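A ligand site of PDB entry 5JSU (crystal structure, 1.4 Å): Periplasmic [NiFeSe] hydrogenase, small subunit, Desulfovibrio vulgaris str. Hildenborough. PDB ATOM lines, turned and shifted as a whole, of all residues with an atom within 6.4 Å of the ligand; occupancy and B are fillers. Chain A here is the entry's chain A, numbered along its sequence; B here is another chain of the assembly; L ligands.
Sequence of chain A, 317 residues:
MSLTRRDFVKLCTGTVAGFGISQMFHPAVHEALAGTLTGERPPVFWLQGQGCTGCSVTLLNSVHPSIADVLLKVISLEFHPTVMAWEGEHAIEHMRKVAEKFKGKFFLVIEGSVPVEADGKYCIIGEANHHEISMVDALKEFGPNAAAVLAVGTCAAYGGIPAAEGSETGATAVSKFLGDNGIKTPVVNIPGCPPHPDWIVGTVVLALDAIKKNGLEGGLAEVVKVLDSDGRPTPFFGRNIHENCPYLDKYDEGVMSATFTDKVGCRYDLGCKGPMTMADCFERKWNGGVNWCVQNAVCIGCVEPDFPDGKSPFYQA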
ATOM      1  N   GLN A  50     -19.829  -7.954 -18.659  1.00  0.00           N
ATOM      2  CA  GLN A  50     -21.264  -7.996 -18.954  1.00  0.00           C
ATOM      3  C   GLN A  50     -21.582  -9.224 -19.796  1.00  0.00           C
ATOM      4  O   GLN A  50     -21.923  -9.140 -20.974  1.00  0.00           O
ATOM      5  CB  GLN A  50     -21.697  -6.727 -19.667  1.00  0.00           C
ATOM      6  CG  GLN A  50     -21.617  -5.498 -18.793  1.00  0.00           C
ATOM      7  CD  GLN A  50     -21.834  -4.254 -19.607  1.00  0.00           C
ATOM      8  OE1 GLN A  50     -21.088  -3.986 -20.553  1.00  0.00           O
ATOM      9  NE2 GLN A  50     -22.861  -3.487 -19.257  1.00  0.00           N
ATOM     10  N   GLY A  51     -21.440 -10.389 -19.170  1.00  0.00           N
ATOM     11  CA  GLY A  51     -21.716 -11.664 -19.805  1.00  0.00           C
ATOM     12  C   GLY A  51     -22.935 -12.329 -19.195  1.00  0.00           C
ATOM     13  O   GLY A  51     -23.458 -11.897 -18.165  1.00  0.00           O
ATOM     14  N   CYS A  52     -23.384 -13.383 -19.861  1.00  0.00           N
ATOM     15  CA  CYS A  52     -24.545 -14.160 -19.411  1.00  0.00           C
ATOM     16  C   CYS A  52     -24.139 -15.541 -18.917  1.00  0.00           C
ATOM     17  O   CYS A  52     -25.010 -16.327 -18.524  1.00  0.00           O
ATOM     18  CB  CYS A  52     -25.610 -14.280 -20.523  1.00  0.00           C
ATOM     19  SG  CYS A  52     -25.264 -15.537 -21.784  1.00  0.00           S
ATOM     20  N   THR A  53     -22.848 -15.859 -18.911  1.00  0.00           N
ATOM     21  CA  THR A  53     -22.279 -17.145 -18.517  1.00  0.00           C
ATOM     22  C   THR A  53     -22.480 -18.179 -19.620  1.00  0.00           C
ATOM     23  O   THR A  53     -22.022 -19.329 -19.498  1.00  0.00           O
ATOM     24  CB  THR A  53     -22.747 -17.575 -17.120  1.00  0.00           C
ATOM     25  OG1 THR A  53     -22.511 -16.490 -16.219  1.00  0.00           O
ATOM     26  CG2 THR A  53     -21.992 -18.798 -16.604  1.00  0.00           C
ATOM     27  N   GLY A  54     -23.083 -17.785 -20.748  1.00  0.00           N
ATOM     28  CA  GLY A  54     -23.263 -18.715 -21.840  1.00  0.00           C
ATOM     29  C   GLY A  54     -21.977 -19.178 -22.493  1.00  0.00           C
ATOM     30  O   GLY A  54     -21.915 -20.284 -23.048  1.00  0.00           O
ATOM     31  N   CYS A  55     -20.942 -18.355 -22.421  1.00  0.00           N
ATOM     32  CA  CYS A  55     -19.665 -18.717 -23.012  1.00  0.00           C
ATOM     33  C   CYS A  55     -18.940 -19.736 -22.132  1.00  0.00           C
ATOM     34  O   CYS A  55     -18.228 -20.606 -22.643  1.00  0.00           O
ATOM     35  CB  CYS A  55     -18.875 -17.440 -23.354  1.00  0.00           C
ATOM     36  SG  CYS A  55     -19.602 -16.393 -24.706  1.00  0.00           S
ATOM     37  N   SER A  56     -19.179 -19.702 -20.807  1.00  0.00           N
ATOM     38  CA  SER A  56     -18.732 -20.776 -19.933  1.00  0.00           C
ATOM     39  C   SER A  56     -19.545 -22.042 -20.152  1.00  0.00           C
ATOM     40  O   SER A  56     -18.992 -23.154 -20.255  1.00  0.00           O
ATOM     41  CB  SER A  56     -18.834 -20.348 -18.467  1.00  0.00           C
ATOM     42  OG  SER A  56     -17.883 -19.360 -18.149  1.00  0.00           O
ATOM     43  N   GLU A 111     -15.147 -12.874 -20.883  1.00  0.00           N
ATOM     44  CA  GLU A 111     -16.519 -13.221 -21.267  1.00  0.00           C
ATOM     45  C   GLU A 111     -17.400 -12.042 -20.886  1.00  0.00           C
ATOM     46  O   GLU A 111     -17.469 -11.674 -19.714  1.00  0.00           O
ATOM     47  CB  GLU A 111     -16.969 -14.485 -20.512  1.00  0.00           C
ATOM     48  CG  GLU A 111     -18.482 -14.832 -20.561  1.00  0.00           C
ATOM     49  CD  GLU A 111     -18.860 -16.174 -19.892  1.00  0.00           C
ATOM     50  OE1 GLU A 111     -18.148 -16.626 -18.967  1.00  0.00           O
ATOM     51  OE2 GLU A 111     -19.903 -16.773 -20.243  1.00  0.00           O
ATOM     52  N   GLY A 112     -18.054 -11.434 -21.886  1.00  0.00           N
ATOM     53  CA  GLY A 112     -18.866 -10.241 -21.703  1.00  0.00           C
ATOM     54  C   GLY A 112     -18.144  -8.965 -22.114  1.00  0.00           C
ATOM     55  O   GLY A 112     -16.923  -8.922 -22.236  1.00  0.00           O
ATOM     56  N   SER A 113     -18.930  -7.902 -22.320  1.00  0.00           N
ATOM     57  CA  SER A 113     -18.381  -6.597 -22.638  1.00  0.00           C
ATOM     58  C   SER A 113     -17.907  -5.858 -21.378  1.00  0.00           C
ATOM     59  O   SER A 113     -18.162  -6.258 -20.235  1.00  0.00           O
ATOM     60  CB  SER A 113     -19.434  -5.766 -23.382  1.00  0.00           C
ATOM     61  OG  SER A 113     -20.665  -5.697 -22.675  1.00  0.00           O
ATOM     62  N   VAL A 152     -13.814 -14.075 -25.662  1.00  0.00           N
ATOM     63  CA  VAL A 152     -14.683 -15.189 -25.966  1.00  0.00           C
ATOM     64  C   VAL A 152     -16.110 -14.675 -25.980  1.00  0.00           C
ATOM     65  O   VAL A 152     -16.561 -14.041 -25.007  1.00  0.00           O
ATOM     66  CB  VAL A 152     -14.482 -16.327 -24.934  1.00  0.00           C
ATOM     67  CG1 VAL A 152     -15.463 -17.434 -25.144  1.00  0.00           C
ATOM     68  CG2 VAL A 152     -13.070 -16.900 -25.049  1.00  0.00           C
ATOM     69  N   GLY A 153     -16.817 -14.942 -27.070  1.00  0.00           N
ATOM     70  CA  GLY A 153     -18.171 -14.492 -27.268  1.00  0.00           C
ATOM     71  C   GLY A 153     -18.235 -13.155 -27.952  1.00  0.00           C
ATOM     72  O   GLY A 153     -17.321 -12.331 -27.891  1.00  0.00           O
ATOM     73  N   THR A 154     -19.358 -12.930 -28.640  1.00  0.00           N
ATOM     74  CA  THR A 154     -19.579 -11.686 -29.359  1.00  0.00           C
ATOM     75  C   THR A 154     -19.621 -10.459 -28.462  1.00  0.00           C
ATOM     76  O   THR A 154     -19.191  -9.387 -28.896  1.00  0.00           O
ATOM     77  CB  THR A 154     -20.842 -11.840 -30.193  1.00  0.00           C
ATOM     78  OG1 THR A 154     -20.540 -12.816 -31.188  1.00  0.00           O
ATOM     79  CG2 THR A 154     -21.270 -10.565 -30.866  1.00  0.00           C
ATOM     80  N   CYS A 155     -20.100 -10.579 -27.215  1.00  0.00           N
ATOM     81  CA  CYS A 155     -20.061  -9.418 -26.322  1.00  0.00           C
ATOM     82  C   CYS A 155     -18.616  -8.930 -26.134  1.00  0.00           C
ATOM     83  O   CYS A 155     -18.321  -7.738 -26.301  1.00  0.00           O
ATOM     84  CB  CYS A 155     -20.650  -9.744 -24.946  1.00  0.00           C
ATOM     85  SG  CYS A 155     -22.358 -10.259 -24.875  1.00  0.00           S
ATOM     86  N   ALA A 156     -17.732  -9.840 -25.726  1.00  0.00           N
ATOM     87  CA  ALA A 156     -16.336  -9.464 -25.517  1.00  0.00           C
ATOM     88  C   ALA A 156     -15.660  -9.070 -26.813  1.00  0.00           C
ATOM     89  O   ALA A 156     -14.891  -8.115 -26.846  1.00  0.00           O
ATOM     90  CB  ALA A 156     -15.577 -10.613 -24.845  1.00  0.00           C
ATOM     91  N   ILE A 161     -24.914  -7.777 -27.537  1.00  0.00           N
ATOM     92  CA  ILE A 161     -26.208  -7.262 -27.069  1.00  0.00           C
ATOM     93  C   ILE A 161     -26.038  -6.149 -26.056  1.00  0.00           C
ATOM     94  O   ILE A 161     -26.756  -5.137 -26.146  1.00  0.00           O
ATOM     95  CB  ILE A 161     -27.105  -8.428 -26.613  1.00  0.00           C
ATOM     96  CG1 ILE A 161     -27.543  -9.227 -27.840  1.00  0.00           C
ATOM     97  CG2 ILE A 161     -28.319  -7.904 -25.846  1.00  0.00           C
ATOM     98  CD1 ILE A 161     -28.261 -10.503 -27.524  1.00  0.00           C
ATOM     99  N   PRO A 162     -25.100  -6.202 -25.101  1.00  0.00           N
ATOM    100  CA  PRO A 162     -24.985  -5.085 -24.146  1.00  0.00           C
ATOM    101  C   PRO A 162     -24.649  -3.755 -24.784  1.00  0.00           C
ATOM    102  O   PRO A 162     -24.911  -2.710 -24.174  1.00  0.00           O
ATOM    103  CB  PRO A 162     -23.886  -5.549 -23.187  1.00  0.00           C
ATOM    104  CG  PRO A 162     -23.984  -7.063 -23.218  1.00  0.00           C
ATOM    105  CD  PRO A 162     -24.287  -7.362 -24.673  1.00  0.00           C
ATOM    106  N   GLY A 192     -19.408 -15.479 -31.465  1.00  0.00           N
ATOM    107  CA  GLY A 192     -20.541 -16.369 -31.335  1.00  0.00           C
ATOM    108  C   GLY A 192     -21.330 -15.985 -30.091  1.00  0.00           C
ATOM    109  O   GLY A 192     -20.776 -15.471 -29.123  1.00  0.00           O
ATOM    110  N   CYS A 193     -22.617 -16.270 -30.108  1.00  0.00           N
ATOM    111  CA  CYS A 193     -23.494 -15.940 -28.992  1.00  0.00           C
ATOM    112  C   CYS A 193     -24.410 -17.127 -28.688  1.00  0.00           C
ATOM    113  O   CYS A 193     -25.593 -17.120 -29.030  1.00  0.00           O
ATOM    114  CB  CYS A 193     -24.285 -14.672 -29.283  1.00  0.00           C
ATOM    115  SG  CYS A 193     -25.111 -13.944 -27.812  1.00  0.00           S
ATOM    116  N   PRO A 194     -23.851 -18.169 -28.066  1.00  0.00           N
ATOM    117  CA  PRO A 194     -22.441 -18.319 -27.682  1.00  0.00           C
ATOM    118  C   PRO A 194     -21.610 -18.916 -28.815  1.00  0.00           C
ATOM    119  O   PRO A 194     -22.138 -19.408 -29.819  1.00  0.00           O
ATOM    120  CB  PRO A 194     -22.528 -19.368 -26.576  1.00  0.00           C
ATOM    121  CG  PRO A 194     -23.614 -20.273 -27.046  1.00  0.00           C
ATOM    122  CD  PRO A 194     -24.625 -19.395 -27.781  1.00  0.00           C
ATOM    123  N   PRO A 195     -20.291 -18.880 -28.654  1.00  0.00           N
ATOM    124  CA  PRO A 195     -19.425 -19.688 -29.529  1.00  0.00           C
ATOM    125  C   PRO A 195     -19.735 -21.169 -29.368  1.00  0.00           C
ATOM    126  O   PRO A 195     -20.255 -21.628 -28.365  1.00  0.00           O
ATOM    127  CB  PRO A 195     -18.023 -19.382 -29.004  1.00  0.00           C
ATOM    128  CG  PRO A 195     -18.152 -18.129 -28.175  1.00  0.00           C
ATOM    129  CD  PRO A 195     -19.535 -18.207 -27.603  1.00  0.00           C
ATOM    130  N   PHE A 307     -23.710  -8.023 -34.767  1.00  0.00           N
ATOM    131  CA  PHE A 307     -24.764  -8.722 -34.027  1.00  0.00           C
ATOM    132  C   PHE A 307     -25.014  -7.991 -32.699  1.00  0.00           C
ATOM    133  O   PHE A 307     -24.076  -7.744 -31.953  1.00  0.00           O
ATOM    134  CB  PHE A 307     -24.374 -10.176 -33.775  1.00  0.00           C
ATOM    135  CG  PHE A 307     -25.418 -10.952 -33.000  1.00  0.00           C
ATOM    136  CD1 PHE A 307     -26.499 -11.506 -33.663  1.00  0.00           C
ATOM    137  CD2 PHE A 307     -25.317 -11.108 -31.620  1.00  0.00           C
ATOM    138  CE1 PHE A 307     -27.474 -12.199 -32.961  1.00  0.00           C
ATOM    139  CE2 PHE A 307     -26.299 -11.798 -30.930  1.00  0.00           C
ATOM    140  CZ  PHE A 307     -27.366 -12.353 -31.602  1.00  0.00           C
ATOM    141  N   ARG B  50     -26.967  -4.723 -17.416  1.00  0.00           N
ATOM    142  CA  ARG B  50     -26.987  -4.610 -18.871  1.00  0.00           C
ATOM    143  C   ARG B  50     -28.165  -3.811 -19.406  1.00  0.00           C
ATOM    144  O   ARG B  50     -27.985  -3.043 -20.354  1.00  0.00           O
ATOM    145  CB  ARG B  50     -26.934  -6.018 -19.522  1.00  0.00           C
ATOM    146  CG  ARG B  50     -25.541  -6.621 -19.398  1.00  0.00           C
ATOM    147  CD  ARG B  50     -25.488  -8.136 -19.637  1.00  0.00           C
ATOM    148  NE  ARG B  50     -26.313  -8.848 -18.686  1.00  0.00           N
ATOM    149  CZ  ARG B  50     -26.791 -10.073 -18.870  1.00  0.00           C
ATOM    150  NH1 ARG B  50     -26.469 -10.774 -19.949  1.00  0.00           N
ATOM    151  NH2 ARG B  50     -27.615 -10.577 -17.973  1.00  0.00           N
ATOM    152  N   PHE B  52     -31.527  -4.990 -20.494  1.00  0.00           N
ATOM    153  CA  PHE B  52     -32.324  -5.581 -21.552  1.00  0.00           C
ATOM    154  C   PHE B  52     -33.662  -4.897 -21.749  1.00  0.00           C
ATOM    155  O   PHE B  52     -34.129  -4.793 -22.881  1.00  0.00           O
ATOM    156  CB  PHE B  52     -32.551  -7.070 -21.266  1.00  0.00           C
ATOM    157  CG  PHE B  52     -31.368  -7.932 -21.604  1.00  0.00           C
ATOM    158  CD1 PHE B  52     -30.250  -7.954 -20.791  1.00  0.00           C
ATOM    159  CD2 PHE B  52     -31.350  -8.686 -22.766  1.00  0.00           C
ATOM    160  CE1 PHE B  52     -29.153  -8.718 -21.114  1.00  0.00           C
ATOM    161  CE2 PHE B  52     -30.265  -9.466 -23.085  1.00  0.00           C
ATOM    162  CZ  PHE B  52     -29.157  -9.475 -22.255  1.00  0.00           C
ATOM    163  N   ARG B  70     -30.280 -14.022 -23.877  1.00  0.00           N
ATOM    164  CA  ARG B  70     -28.946 -13.609 -23.506  1.00  0.00           C
ATOM    165  C   ARG B  70     -28.913 -12.960 -22.130  1.00  0.00           C
ATOM    166  O   ARG B  70     -27.838 -12.555 -21.673  1.00  0.00           O
ATOM    167  CB  ARG B  70     -28.344 -12.714 -24.585  1.00  0.00           C
ATOM    168  CG  ARG B  70     -27.820 -13.492 -25.803  1.00  0.00           C
ATOM    169  CD  ARG B  70     -28.900 -14.034 -26.732  1.00  0.00           C
ATOM    170  NE  ARG B  70     -28.292 -14.783 -27.825  1.00  0.00           N
ATOM    171  CZ  ARG B  70     -28.934 -15.550 -28.680  1.00  0.00           C
ATOM    172  NH1 ARG B  70     -30.269 -15.620 -28.663  1.00  0.00           N
ATOM    173  NH2 ARG B  70     -28.241 -16.241 -29.584  1.00  0.00           N
ATOM    174  N   ILE B  71     -30.053 -12.867 -21.455  1.00  0.00           N
ATOM    175  CA  ILE B  71     -30.016 -12.548 -20.038  1.00  0.00           C
ATOM    176  C   ILE B  71     -29.231 -13.605 -19.277  1.00  0.00           C
ATOM    177  O   ILE B  71     -28.533 -13.293 -18.298  1.00  0.00           O
ATOM    178  CB  ILE B  71     -31.457 -12.418 -19.494  1.00  0.00           C
ATOM    179  CG1 ILE B  71     -32.115 -11.159 -20.075  1.00  0.00           C
ATOM    180  CG2 ILE B  71     -31.450 -12.411 -17.962  1.00  0.00           C
ATOM    181  CD1 ILE B  71     -33.618 -11.105 -19.880  1.00  0.00           C
ATOM    182  N   CYS B  72     -29.410 -14.875 -19.633  1.00  0.00           N
ATOM    183  CA  CYS B  72     -28.715 -15.937 -18.920  1.00  0.00           C
ATOM    184  C   CYS B  72     -28.405 -17.075 -19.864  1.00  0.00           C
ATOM    185  O   CYS B  72     -29.279 -17.563 -20.594  1.00  0.00           O
ATOM    186  CB  CYS B  72     -29.551 -16.471 -17.762  1.00  0.00           C
ATOM    187  SG  CYS B  72     -31.022 -17.367 -18.320  1.00  0.00           S
ATOM    188  N   GLY B  73     -27.162 -17.515 -19.824  1.00  0.00           N
ATOM    189  CA  GLY B  73     -26.677 -18.685 -20.545  1.00  0.00           C
ATOM    190  C   GLY B  73     -26.950 -20.015 -19.860  1.00  0.00           C
ATOM    191  O   GLY B  73     -26.850 -21.058 -20.515  1.00  0.00           O
ATOM    192  N   PRO B 181     -26.307 -23.353 -25.314  1.00  0.00           N
ATOM    193  CA  PRO B 181     -27.198 -22.242 -24.977  1.00  0.00           C
ATOM    194  C   PRO B 181     -27.785 -21.545 -26.197  1.00  0.00           C
ATOM    195  O   PRO B 181     -27.225 -21.573 -27.308  1.00  0.00           O
ATOM    196  CB  PRO B 181     -26.277 -21.255 -24.230  1.00  0.00           C
ATOM    197  CG  PRO B 181     -25.178 -22.104 -23.676  1.00  0.00           C
ATOM    198  CD  PRO B 181     -24.968 -23.176 -24.723  1.00  0.00           C
ATOM    199  N   HIS B 182     -28.944 -20.930 -25.938  1.00  0.00           N
ATOM    200  CA  HIS B 182     -29.635 -20.001 -26.809  1.00  0.00           C
ATOM    201  C   HIS B 182     -30.354 -20.712 -27.950  1.00  0.00           C
ATOM    202  O   HIS B 182     -29.897 -20.757 -29.096  1.00  0.00           O
ATOM    203  CB  HIS B 182     -28.747 -18.834 -27.234  1.00  0.00           C
ATOM    204  CG  HIS B 182     -28.185 -18.082 -26.067  1.00  0.00           C
ATOM    205  ND1 HIS B 182     -28.811 -18.076 -24.828  1.00  0.00           N
ATOM    206  CD2 HIS B 182     -27.041 -17.392 -25.914  1.00  0.00           C
ATOM    207  CE1 HIS B 182     -28.081 -17.370 -23.989  1.00  0.00           C
ATOM    208  NE2 HIS B 182     -26.996 -16.953 -24.617  1.00  0.00           N
HETATM  209 FE1  LIG L   1     -23.775 -14.593 -23.246  1.00  0.00          FE
HETATM  210 FE2  LIG L   1     -22.392 -12.567 -24.444  1.00  0.00          FE
HETATM  211 FE3  LIG L   1     -23.757 -14.276 -25.969  1.00  0.00          FE
HETATM  212 FE4  LIG L   1     -21.499 -15.203 -24.539  1.00  0.00          FE
HETATM  213  S1  LIG L   1     -21.574 -13.684 -26.257  1.00  0.00           S
HETATM  214  S2  LIG L   1     -23.547 -16.236 -24.818  1.00  0.00           S
HETATM  215  S3  LIG L   1     -21.622 -13.860 -22.687  1.00  0.00           S
HETATM  216  S4  LIG L   1     -24.681 -12.864 -24.404  1.00  0.00           S
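S2 of the ligand lies close to NE2 of His 182 of chain B (3.5 Å). An iron atom (FE4) of the ligand is bound by the side-chain sulfur (SG) of Cys 55, 2.2 Å away. A sulfur (S3) of the ligand lies close to the backbone NH (N) of Cys 52 of chain A, at 3.4 Å. An iron atom (FE3) of the ligand is bound by the side-chain sulfur (SG) of Cys 193. The backbone NH (N) of Cys 155 sits close to a sulfur (S1) of the ligand (3.6 Å). S1 of the ligand lies close to N of Thr 154. SG of Cys 155 is bound to FE2 of the ligand, 2.3 Å away. The side-chain sulfur of Cys 52 of chain A binds an iron atom (FE1) of the ligand (2.3 Å).
O of Cys 52 of chain A lies within hydrogen-bond range of N of Gly 73 of chain B (2.8 Å). The side-chain carboxylate of Glu 111 lies close to the backbone NH of Thr 53 (3.4 Å). The backbone NH of Cys 55 lies within hydrogen-bond range of the side-chain carboxylate of Glu 111 (2.9 Å). SG of Cys 52 of chain A lies close to NE2 of His 182 of chain B (3.6 Å). N of Gly 54 sits at hydrogen-bond distance from OE2 of Glu 111 (3.4 Å). The guanidinium group of Arg 50 of chain B is in hydrogen-bond range of the backbone carbonyl oxygen of Arg 70 of chain B, 2.8 Å away. N of Gly 192 sits at hydrogen-bond distance from OG1 of Thr 154, at 2.9 Å. The backbone NH (N) of Gly 54 sits close to the side-chain sulfur (SG) of Cys 52 of chain A (3.3 Å).
A sulfur (S1) of the ligand sits close to the backbone carbonyl oxygen of Gly 192 (3.5 Å). The backbone nitrogen (N) of Pro 194 sits close to a sulfur (S2) of the ligand (3.8 Å). Residues that only touch the ligand: Arg 70 of chain B (3.5 Å), Gly 51 (3.6 Å), Gly 153 (3.6 Å), Gly 54 (3.9 Å) and Glu 111 (3.9 Å). Hydrophobic or aromatic side chains within 4 Å of the ligand: Pro 194 and His 182 of chain B. Within 4 Å of the ligand: Gly 51, Cys 52 of chain A, Gly 54, Cys 55, Glu 111, Gly 153, Thr 154, Cys 155, Gly 192, Cys 193, Pro 194, Arg 70 of chain B and His 182 of chain B. The nearest printed residue that does not touch the ligand is Gly 112 (4.4 Å).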
